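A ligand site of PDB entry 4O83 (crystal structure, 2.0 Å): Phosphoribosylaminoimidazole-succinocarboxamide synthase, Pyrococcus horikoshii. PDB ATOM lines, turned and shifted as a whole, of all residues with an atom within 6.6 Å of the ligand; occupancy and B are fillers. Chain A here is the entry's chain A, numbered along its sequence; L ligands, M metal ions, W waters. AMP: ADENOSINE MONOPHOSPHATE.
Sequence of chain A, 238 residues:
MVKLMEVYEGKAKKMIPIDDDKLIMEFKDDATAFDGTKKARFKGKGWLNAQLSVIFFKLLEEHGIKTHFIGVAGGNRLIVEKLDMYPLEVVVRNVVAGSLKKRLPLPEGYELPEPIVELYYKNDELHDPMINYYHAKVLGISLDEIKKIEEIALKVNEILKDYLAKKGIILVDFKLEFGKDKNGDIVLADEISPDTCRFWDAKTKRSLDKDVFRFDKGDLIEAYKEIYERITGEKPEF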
ATOM      1  N   ALA A  12      -7.184 -13.888   9.631  1.00  0.00           N
ATOM      2  CA  ALA A  12      -6.488 -13.602  10.923  1.00  0.00           C
ATOM      3  C   ALA A  12      -6.018 -12.145  11.043  1.00  0.00           C
ATOM      4  O   ALA A  12      -5.537 -11.744  12.104  1.00  0.00           O
ATOM      5  CB  ALA A  12      -5.344 -14.566  11.141  1.00  0.00           C
ATOM      6  N   LYS A  13      -6.159 -11.380   9.964  1.00  0.00           N
ATOM      7  CA  LYS A  13      -5.945  -9.916   9.981  1.00  0.00           C
ATOM      8  C   LYS A  13      -7.141  -9.192   9.370  1.00  0.00           C
ATOM      9  O   LYS A  13      -7.803  -9.722   8.470  1.00  0.00           O
ATOM     10  CB  LYS A  13      -4.659  -9.499   9.233  1.00  0.00           C
ATOM     11  CG  LYS A  13      -3.373 -10.111   9.757  1.00  0.00           C
ATOM     12  CD  LYS A  13      -2.128  -9.429   9.199  1.00  0.00           C
ATOM     13  CE  LYS A  13      -1.951  -9.626   7.696  1.00  0.00           C
ATOM     14  NZ  LYS A  13      -1.995 -11.046   7.281  1.00  0.00           N
ATOM     15  N   LYS A  14      -7.388  -7.982   9.845  1.00  0.00           N
ATOM     16  CA  LYS A  14      -8.385  -7.111   9.215  1.00  0.00           C
ATOM     17  C   LYS A  14      -7.685  -5.833   8.747  1.00  0.00           C
ATOM     18  O   LYS A  14      -6.963  -5.195   9.529  1.00  0.00           O
ATOM     19  CB  LYS A  14      -9.515  -6.807  10.189  1.00  0.00           C
ATOM     20  N   MET A  15      -7.875  -5.477   7.477  1.00  0.00           N
ATOM     21  CA  MET A  15      -7.300  -4.265   6.898  1.00  0.00           C
ATOM     22  C   MET A  15      -8.367  -3.218   6.831  1.00  0.00           C
ATOM     23  O   MET A  15      -9.370  -3.379   6.129  1.00  0.00           O
ATOM     24  CB  MET A  15      -6.738  -4.478   5.492  1.00  0.00           C
ATOM     25  CG  MET A  15      -5.860  -5.721   5.377  1.00  0.00           C
ATOM     26  SD  MET A  15      -4.248  -5.549   6.511  1.00  0.00           S
ATOM     27  CE  MET A  15      -3.079  -4.620   5.237  1.00  0.00           C
ATOM     28  N   LEU A  23      -3.409   2.517   5.990  1.00  0.00           N
ATOM     29  CA  LEU A  23      -4.435   1.686   6.559  1.00  0.00           C
ATOM     30  C   LEU A  23      -4.021   1.064   7.893  1.00  0.00           C
ATOM     31  O   LEU A  23      -2.853   1.128   8.309  1.00  0.00           O
ATOM     32  CB  LEU A  23      -4.892   0.622   5.553  1.00  0.00           C
ATOM     33  CG  LEU A  23      -3.906  -0.388   4.981  1.00  0.00           C
ATOM     34  CD1 LEU A  23      -3.950  -1.612   5.868  1.00  0.00           C
ATOM     35  CD2 LEU A  23      -4.288  -0.746   3.550  1.00  0.00           C
ATOM     36  N   MET A  25      -3.774  -2.356  10.042  1.00  0.00           N
ATOM     37  CA  MET A  25      -3.715  -3.814   9.973  1.00  0.00           C
ATOM     38  C   MET A  25      -4.004  -4.288  11.361  1.00  0.00           C
ATOM     39  O   MET A  25      -3.203  -4.086  12.279  1.00  0.00           O
ATOM     40  CB  MET A  25      -2.300  -4.190   9.509  1.00  0.00           C
ATOM     41  CG  MET A  25      -2.071  -5.697   9.467  1.00  0.00           C
ATOM     42  SD  MET A  25      -0.502  -6.008   8.307  1.00  0.00           S
ATOM     43  CE  MET A  25       0.916  -5.264   9.433  1.00  0.00           C
ATOM     44  N   HIS A  68       6.220  -1.549   4.728  1.00  0.00           N
ATOM     45  CA  HIS A  68       5.003  -0.762   4.812  1.00  0.00           C
ATOM     46  C   HIS A  68       4.742  -0.219   6.195  1.00  0.00           C
ATOM     47  O   HIS A  68       3.828   0.572   6.388  1.00  0.00           O
ATOM     48  CB  HIS A  68       3.808  -1.542   4.269  1.00  0.00           C
ATOM     49  CG  HIS A  68       3.364  -2.701   5.138  1.00  0.00           C
ATOM     50  ND1 HIS A  68       2.144  -3.253   5.045  1.00  0.00           N
ATOM     51  CD2 HIS A  68       4.028  -3.415   6.142  1.00  0.00           C
ATOM     52  CE1 HIS A  68       2.027  -4.268   5.921  1.00  0.00           C
ATOM     53  NE2 HIS A  68       3.188  -4.377   6.584  1.00  0.00           N
ATOM     54  N   VAL A  80      -0.011   1.040   8.527  1.00  0.00           N
ATOM     55  CA  VAL A  80       0.863   0.698   7.419  1.00  0.00           C
ATOM     56  C   VAL A  80       0.477   1.517   6.196  1.00  0.00           C
ATOM     57  O   VAL A  80      -0.676   1.975   6.046  1.00  0.00           O
ATOM     58  CB  VAL A  80       0.827  -0.817   7.088  1.00  0.00           C
ATOM     59  CG1 VAL A  80       1.345  -1.631   8.263  1.00  0.00           C
ATOM     60  CG2 VAL A  80      -0.574  -1.270   6.677  1.00  0.00           C
ATOM     61  N   GLU A  81       1.456   1.741   5.326  1.00  0.00           N
ATOM     62  CA  GLU A  81       1.203   2.473   4.099  1.00  0.00           C
ATOM     63  C   GLU A  81       0.507   1.570   3.081  1.00  0.00           C
ATOM     64  O   GLU A  81       0.836   0.380   2.967  1.00  0.00           O
ATOM     65  CB  GLU A  81       2.466   3.127   3.557  1.00  0.00           C
ATOM     66  CG  GLU A  81       3.516   2.197   2.994  1.00  0.00           C
ATOM     67  CD  GLU A  81       4.618   2.955   2.282  1.00  0.00           C
ATOM     68  OE1 GLU A  81       5.812   2.708   2.587  1.00  0.00           O
ATOM     69  OE2 GLU A  81       4.308   3.802   1.423  1.00  0.00           O
ATOM     70  N   LYS A  82      -0.465   2.147   2.377  1.00  0.00           N
ATOM     71  CA  LYS A  82      -1.260   1.385   1.419  1.00  0.00           C
ATOM     72  C   LYS A  82      -0.432   1.202   0.159  1.00  0.00           C
ATOM     73  O   LYS A  82       0.195   2.130  -0.338  1.00  0.00           O
ATOM     74  CB  LYS A  82      -2.605   2.074   1.129  1.00  0.00           C
ATOM     75  CG  LYS A  82      -3.597   1.180   0.400  1.00  0.00           C
ATOM     76  CD  LYS A  82      -5.034   1.661   0.580  1.00  0.00           C
ATOM     77  N   LEU A  83      -0.406  -0.037  -0.319  1.00  0.00           N
ATOM     78  CA  LEU A  83       0.421  -0.396  -1.463  1.00  0.00           C
ATOM     79  C   LEU A  83      -0.428  -0.990  -2.585  1.00  0.00           C
ATOM     80  O   LEU A  83      -1.512  -1.533  -2.349  1.00  0.00           O
ATOM     81  CB  LEU A  83       1.511  -1.390  -1.042  1.00  0.00           C
ATOM     82  CG  LEU A  83       2.511  -0.963   0.030  1.00  0.00           C
ATOM     83  CD1 LEU A  83       3.377  -2.150   0.399  1.00  0.00           C
ATOM     84  CD2 LEU A  83       3.370   0.199  -0.449  1.00  0.00           C
ATOM     85  N   ASP A  84       0.109  -0.870  -3.798  1.00  0.00           N
ATOM     86  CA  ASP A  84      -0.362  -1.616  -4.948  1.00  0.00           C
ATOM     87  C   ASP A  84       0.325  -2.984  -4.893  1.00  0.00           C
ATOM     88  O   ASP A  84       1.491  -3.111  -5.273  1.00  0.00           O
ATOM     89  CB  ASP A  84       0.010  -0.846  -6.220  1.00  0.00           C
ATOM     90  CG  ASP A  84      -0.447  -1.538  -7.483  1.00  0.00           C
ATOM     91  OD1 ASP A  84      -1.545  -2.128  -7.488  1.00  0.00           O
ATOM     92  OD2 ASP A  84       0.315  -1.482  -8.478  1.00  0.00           O
ATOM     93  N   MET A  85      -0.393  -3.991  -4.392  1.00  0.00           N
ATOM     94  CA  MET A  85       0.217  -5.287  -4.033  1.00  0.00           C
ATOM     95  C   MET A  85       0.542  -6.126  -5.244  1.00  0.00           C
ATOM     96  O   MET A  85      -0.253  -6.210  -6.182  1.00  0.00           O
ATOM     97  CB  MET A  85      -0.710  -6.125  -3.152  1.00  0.00           C
ATOM     98  CG  MET A  85      -1.027  -5.519  -1.782  1.00  0.00           C
ATOM     99  SD  MET A  85       0.607  -5.292  -0.691  1.00  0.00           S
ATOM    100  CE  MET A  85       0.967  -7.222  -0.468  1.00  0.00           C
ATOM    101  N   TYR A  86       1.701  -6.771  -5.233  1.00  0.00           N
ATOM    102  CA  TYR A  86       1.969  -7.856  -6.193  1.00  0.00           C
ATOM    103  C   TYR A  86       1.155  -9.091  -5.808  1.00  0.00           C
ATOM    104  O   TYR A  86       1.004  -9.383  -4.618  1.00  0.00           O
ATOM    105  CB  TYR A  86       3.445  -8.195  -6.268  1.00  0.00           C
ATOM    106  CG  TYR A  86       4.306  -7.107  -6.877  1.00  0.00           C
ATOM    107  CD1 TYR A  86       4.427  -6.979  -8.262  1.00  0.00           C
ATOM    108  CD2 TYR A  86       4.996  -6.224  -6.061  1.00  0.00           C
ATOM    109  CE1 TYR A  86       5.226  -5.996  -8.818  1.00  0.00           C
ATOM    110  CE2 TYR A  86       5.798  -5.243  -6.603  1.00  0.00           C
ATOM    111  CZ  TYR A  86       5.905  -5.129  -7.979  1.00  0.00           C
ATOM    112  OH  TYR A  86       6.699  -4.135  -8.489  1.00  0.00           O
ATOM    113  N   LEU A  88       1.524 -12.071  -5.264  1.00  0.00           N
ATOM    114  CA  LEU A  88       2.498 -13.098  -4.953  1.00  0.00           C
ATOM    115  C   LEU A  88       2.597 -13.397  -3.466  1.00  0.00           C
ATOM    116  O   LEU A  88       2.410 -12.525  -2.612  1.00  0.00           O
ATOM    117  CB  LEU A  88       3.887 -12.663  -5.423  1.00  0.00           C
ATOM    118  CG  LEU A  88       4.178 -12.354  -6.898  1.00  0.00           C
ATOM    119  CD1 LEU A  88       5.595 -11.824  -7.062  1.00  0.00           C
ATOM    120  CD2 LEU A  88       3.957 -13.582  -7.776  1.00  0.00           C
ATOM    121  N   LYS A 122      -0.708 -15.715  -5.719  1.00  0.00           N
ATOM    122  CA  LYS A 122      -1.632 -15.520  -4.621  1.00  0.00           C
ATOM    123  C   LYS A 122      -3.037 -15.569  -5.164  1.00  0.00           C
ATOM    124  O   LYS A 122      -3.489 -14.607  -5.790  1.00  0.00           O
ATOM    125  CB  LYS A 122      -1.327 -14.206  -3.904  1.00  0.00           C
ATOM    126  CG  LYS A 122      -1.973 -14.042  -2.537  1.00  0.00           C
ATOM    127  CD  LYS A 122      -1.528 -12.724  -1.890  1.00  0.00           C
ATOM    128  CE  LYS A 122      -2.307 -12.435  -0.624  1.00  0.00           C
ATOM    129  NZ  LYS A 122      -2.092 -13.484   0.402  1.00  0.00           N
ATOM    130  N   GLU A 177       5.235 -10.871   1.355  1.00  0.00           N
ATOM    131  CA  GLU A 177       4.459 -10.206   0.325  1.00  0.00           C
ATOM    132  C   GLU A 177       4.984  -8.793   0.112  1.00  0.00           C
ATOM    133  O   GLU A 177       5.540  -8.161   1.041  1.00  0.00           O
ATOM    134  CB  GLU A 177       2.964 -10.171   0.696  1.00  0.00           C
ATOM    135  CG  GLU A 177       2.433 -11.542   1.095  1.00  0.00           C
ATOM    136  CD  GLU A 177       0.915 -11.629   1.236  1.00  0.00           C
ATOM    137  OE1 GLU A 177       0.190 -10.695   0.804  1.00  0.00           O
ATOM    138  OE2 GLU A 177       0.450 -12.663   1.744  1.00  0.00           O
ATOM    139  N   VAL A 187       8.061  -2.463  -1.934  1.00  0.00           N
ATOM    140  CA  VAL A 187       7.968  -2.303  -0.479  1.00  0.00           C
ATOM    141  C   VAL A 187       7.476  -3.598   0.179  1.00  0.00           C
ATOM    142  O   VAL A 187       6.447  -4.150  -0.226  1.00  0.00           O
ATOM    143  CB  VAL A 187       7.011  -1.120  -0.129  1.00  0.00           C
ATOM    144  CG1 VAL A 187       6.796  -1.009   1.374  1.00  0.00           C
ATOM    145  CG2 VAL A 187       7.569   0.178  -0.683  1.00  0.00           C
ATOM    146  N   LEU A 188       8.193  -4.069   1.193  1.00  0.00           N
ATOM    147  CA  LEU A 188       7.795  -5.266   1.942  1.00  0.00           C
ATOM    148  C   LEU A 188       6.523  -5.004   2.759  1.00  0.00           C
ATOM    149  O   LEU A 188       6.398  -3.980   3.433  1.00  0.00           O
ATOM    150  CB  LEU A 188       8.930  -5.753   2.845  1.00  0.00           C
ATOM    151  CG  LEU A 188       8.698  -7.006   3.694  1.00  0.00           C
ATOM    152  CD1 LEU A 188       8.504  -8.241   2.825  1.00  0.00           C
ATOM    153  CD2 LEU A 188       9.855  -7.198   4.669  1.00  0.00           C
ATOM    154  N   ALA A 189       5.573  -5.933   2.690  1.00  0.00           N
ATOM    155  CA  ALA A 189       4.244  -5.718   3.232  1.00  0.00           C
ATOM    156  C   ALA A 189       3.769  -6.848   4.146  1.00  0.00           C
ATOM    157  O   ALA A 189       4.568  -7.631   4.655  1.00  0.00           O
ATOM    158  CB  ALA A 189       3.262  -5.534   2.079  1.00  0.00           C
ATOM    159  N   ASP A 190       2.451  -6.909   4.330  1.00  0.00           N
ATOM    160  CA  ASP A 190       1.766  -7.947   5.119  1.00  0.00           C
ATOM    161  C   ASP A 190       2.308  -8.068   6.550  1.00  0.00           C
ATOM    162  O   ASP A 190       2.465  -7.073   7.233  1.00  0.00           O
ATOM    163  CB  ASP A 190       1.801  -9.286   4.377  1.00  0.00           C
ATOM    164  CG  ASP A 190       0.696 -10.206   4.816  1.00  0.00           C
ATOM    165  OD1 ASP A 190       0.999 -11.306   5.323  1.00  0.00           O
ATOM    166  OD2 ASP A 190      -0.471  -9.840   4.661  1.00  0.00           O
ATOM    167  N   GLU A 191       2.590  -9.292   6.999  1.00  0.00           N
ATOM    168  CA  GLU A 191       3.079  -9.523   8.367  1.00  0.00           C
ATOM    169  C   GLU A 191       4.342 -10.372   8.369  1.00  0.00           C
ATOM    170  O   GLU A 191       4.660 -11.033   7.385  1.00  0.00           O
ATOM    171  CB  GLU A 191       2.001 -10.192   9.234  1.00  0.00           C
ATOM    172  CG  GLU A 191       1.726 -11.627   8.833  1.00  0.00           C
ATOM    173  CD  GLU A 191       0.626 -12.282   9.619  1.00  0.00           C
ATOM    174  OE1 GLU A 191       0.830 -12.543  10.829  1.00  0.00           O
ATOM    175  OE2 GLU A 191      -0.437 -12.544   9.014  1.00  0.00           O
HETATM  176  P   AMP L   1      -5.222 -11.570   5.243  1.00  0.00           P
HETATM  177  O1P AMP L   1      -5.388 -12.399   3.969  1.00  0.00           O
HETATM  178  O2P AMP L   1      -4.512 -12.264   6.377  1.00  0.00           O
HETATM  179  O3P AMP L   1      -6.504 -10.869   5.658  1.00  0.00           O
HETATM  180  O5' AMP L   1      -4.182 -10.402   4.823  1.00  0.00           O
HETATM  181  C5' AMP L   1      -4.527  -9.025   4.674  1.00  0.00           C
HETATM  182  C4' AMP L   1      -4.552  -8.637   3.194  1.00  0.00           C
HETATM  183  O4' AMP L   1      -4.008  -7.318   2.991  1.00  0.00           O
HETATM  184  C3' AMP L   1      -3.735  -9.570   2.322  1.00  0.00           C
HETATM  185  O3' AMP L   1      -4.464  -9.713   1.099  1.00  0.00           O
HETATM  186  C2' AMP L   1      -2.456  -8.812   2.059  1.00  0.00           C
HETATM  187  O2' AMP L   1      -1.898  -9.184   0.793  1.00  0.00           O
HETATM  188  C1' AMP L   1      -2.943  -7.375   2.036  1.00  0.00           C
HETATM  189  N9  AMP L   1      -1.907  -6.403   2.446  1.00  0.00           N
HETATM  190  C8  AMP L   1      -0.941  -6.604   3.341  1.00  0.00           C
HETATM  191  N7  AMP L   1      -0.184  -5.500   3.498  1.00  0.00           N
HETATM  192  C5  AMP L   1      -0.691  -4.541   2.694  1.00  0.00           C
HETATM  193  C6  AMP L   1      -0.381  -3.124   2.371  1.00  0.00           C
HETATM  194  N6  AMP L   1       0.645  -2.483   2.943  1.00  0.00           N
HETATM  195  N1  AMP L   1      -1.161  -2.492   1.462  1.00  0.00           N
HETATM  196  C2  AMP L   1      -2.205  -3.105   0.875  1.00  0.00           C
HETATM  197  N3  AMP L   1      -2.538  -4.388   1.119  1.00  0.00           N
HETATM  198  C4  AMP L   1      -1.833  -5.143   1.996  1.00  0.00           C
HETATM  199 CD    CD M   1      -2.786 -13.638   4.598  1.00  0.00          CD
HETATM  200  O   HOH W   1      -3.777 -15.231   6.830  1.00  0.00           O
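NZ of Lys 13 is in salt-bridge range of O2P of the ligand.
N of Asp 190 lies within hydrogen-bond range of N7 of the ligand (3.1 Å).
A ring nitrogen (ND1) of His 68 sits at hydrogen-bond distance from a nitrogen (N6) of the ligand (2.7 Å).
The side-chain carboxylate (OE1) of Glu 177 is in hydrogen-bond range of an oxygen (O2') of the ligand.
O of Glu 81 is in hydrogen-bond range of N6 of the ligand (2.9 Å).
N of Leu 83 is in hydrogen-bond range of N1 of the ligand.
The backbone carbonyl oxygen (O) of Glu 177 lies within hydrogen-bond range of the backbone NH (N) of Ala 189 (2.8 Å).
OE2 of Glu 177 lies within salt-bridge range of NZ of Lys 122 (3.0 Å).
The side-chain amino group of Lys 13 lies within salt-bridge range of the side-chain carboxylate of Glu 191 (2.8 Å).
NE2 of His 68 lies within hydrogen-bond range of O of Asp 190, at 2.9 Å.
N of His 68 is in hydrogen-bond range of O of Leu 188.
OD2 of Asp 190 lies within salt-bridge range of NZ of Lys 13 (3.3 Å).
The backbone carbonyl oxygen of His 68 is in hydrogen-bond range of the backbone NH of Glu 81.
The side-chain sulfur (SD) of Met 85 lies close to a nitrogen (N3) of the ligand (3.7 Å).
Met 15 touches the ligand (CG to O4', 3.4 Å).
CA of Lys 82 touches N1 of the ligand, 3.9 Å away.
Lys 122 touches the ligand (CE to O2', 3.6 Å).
Ala 189 touches the ligand (CB to N7, 3.7 Å).
Of the 22 residues printed, 11 come within 4 Å of the ligand.
Along chain A the residues within 4 Å of the ligand span positions 13 to 190.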
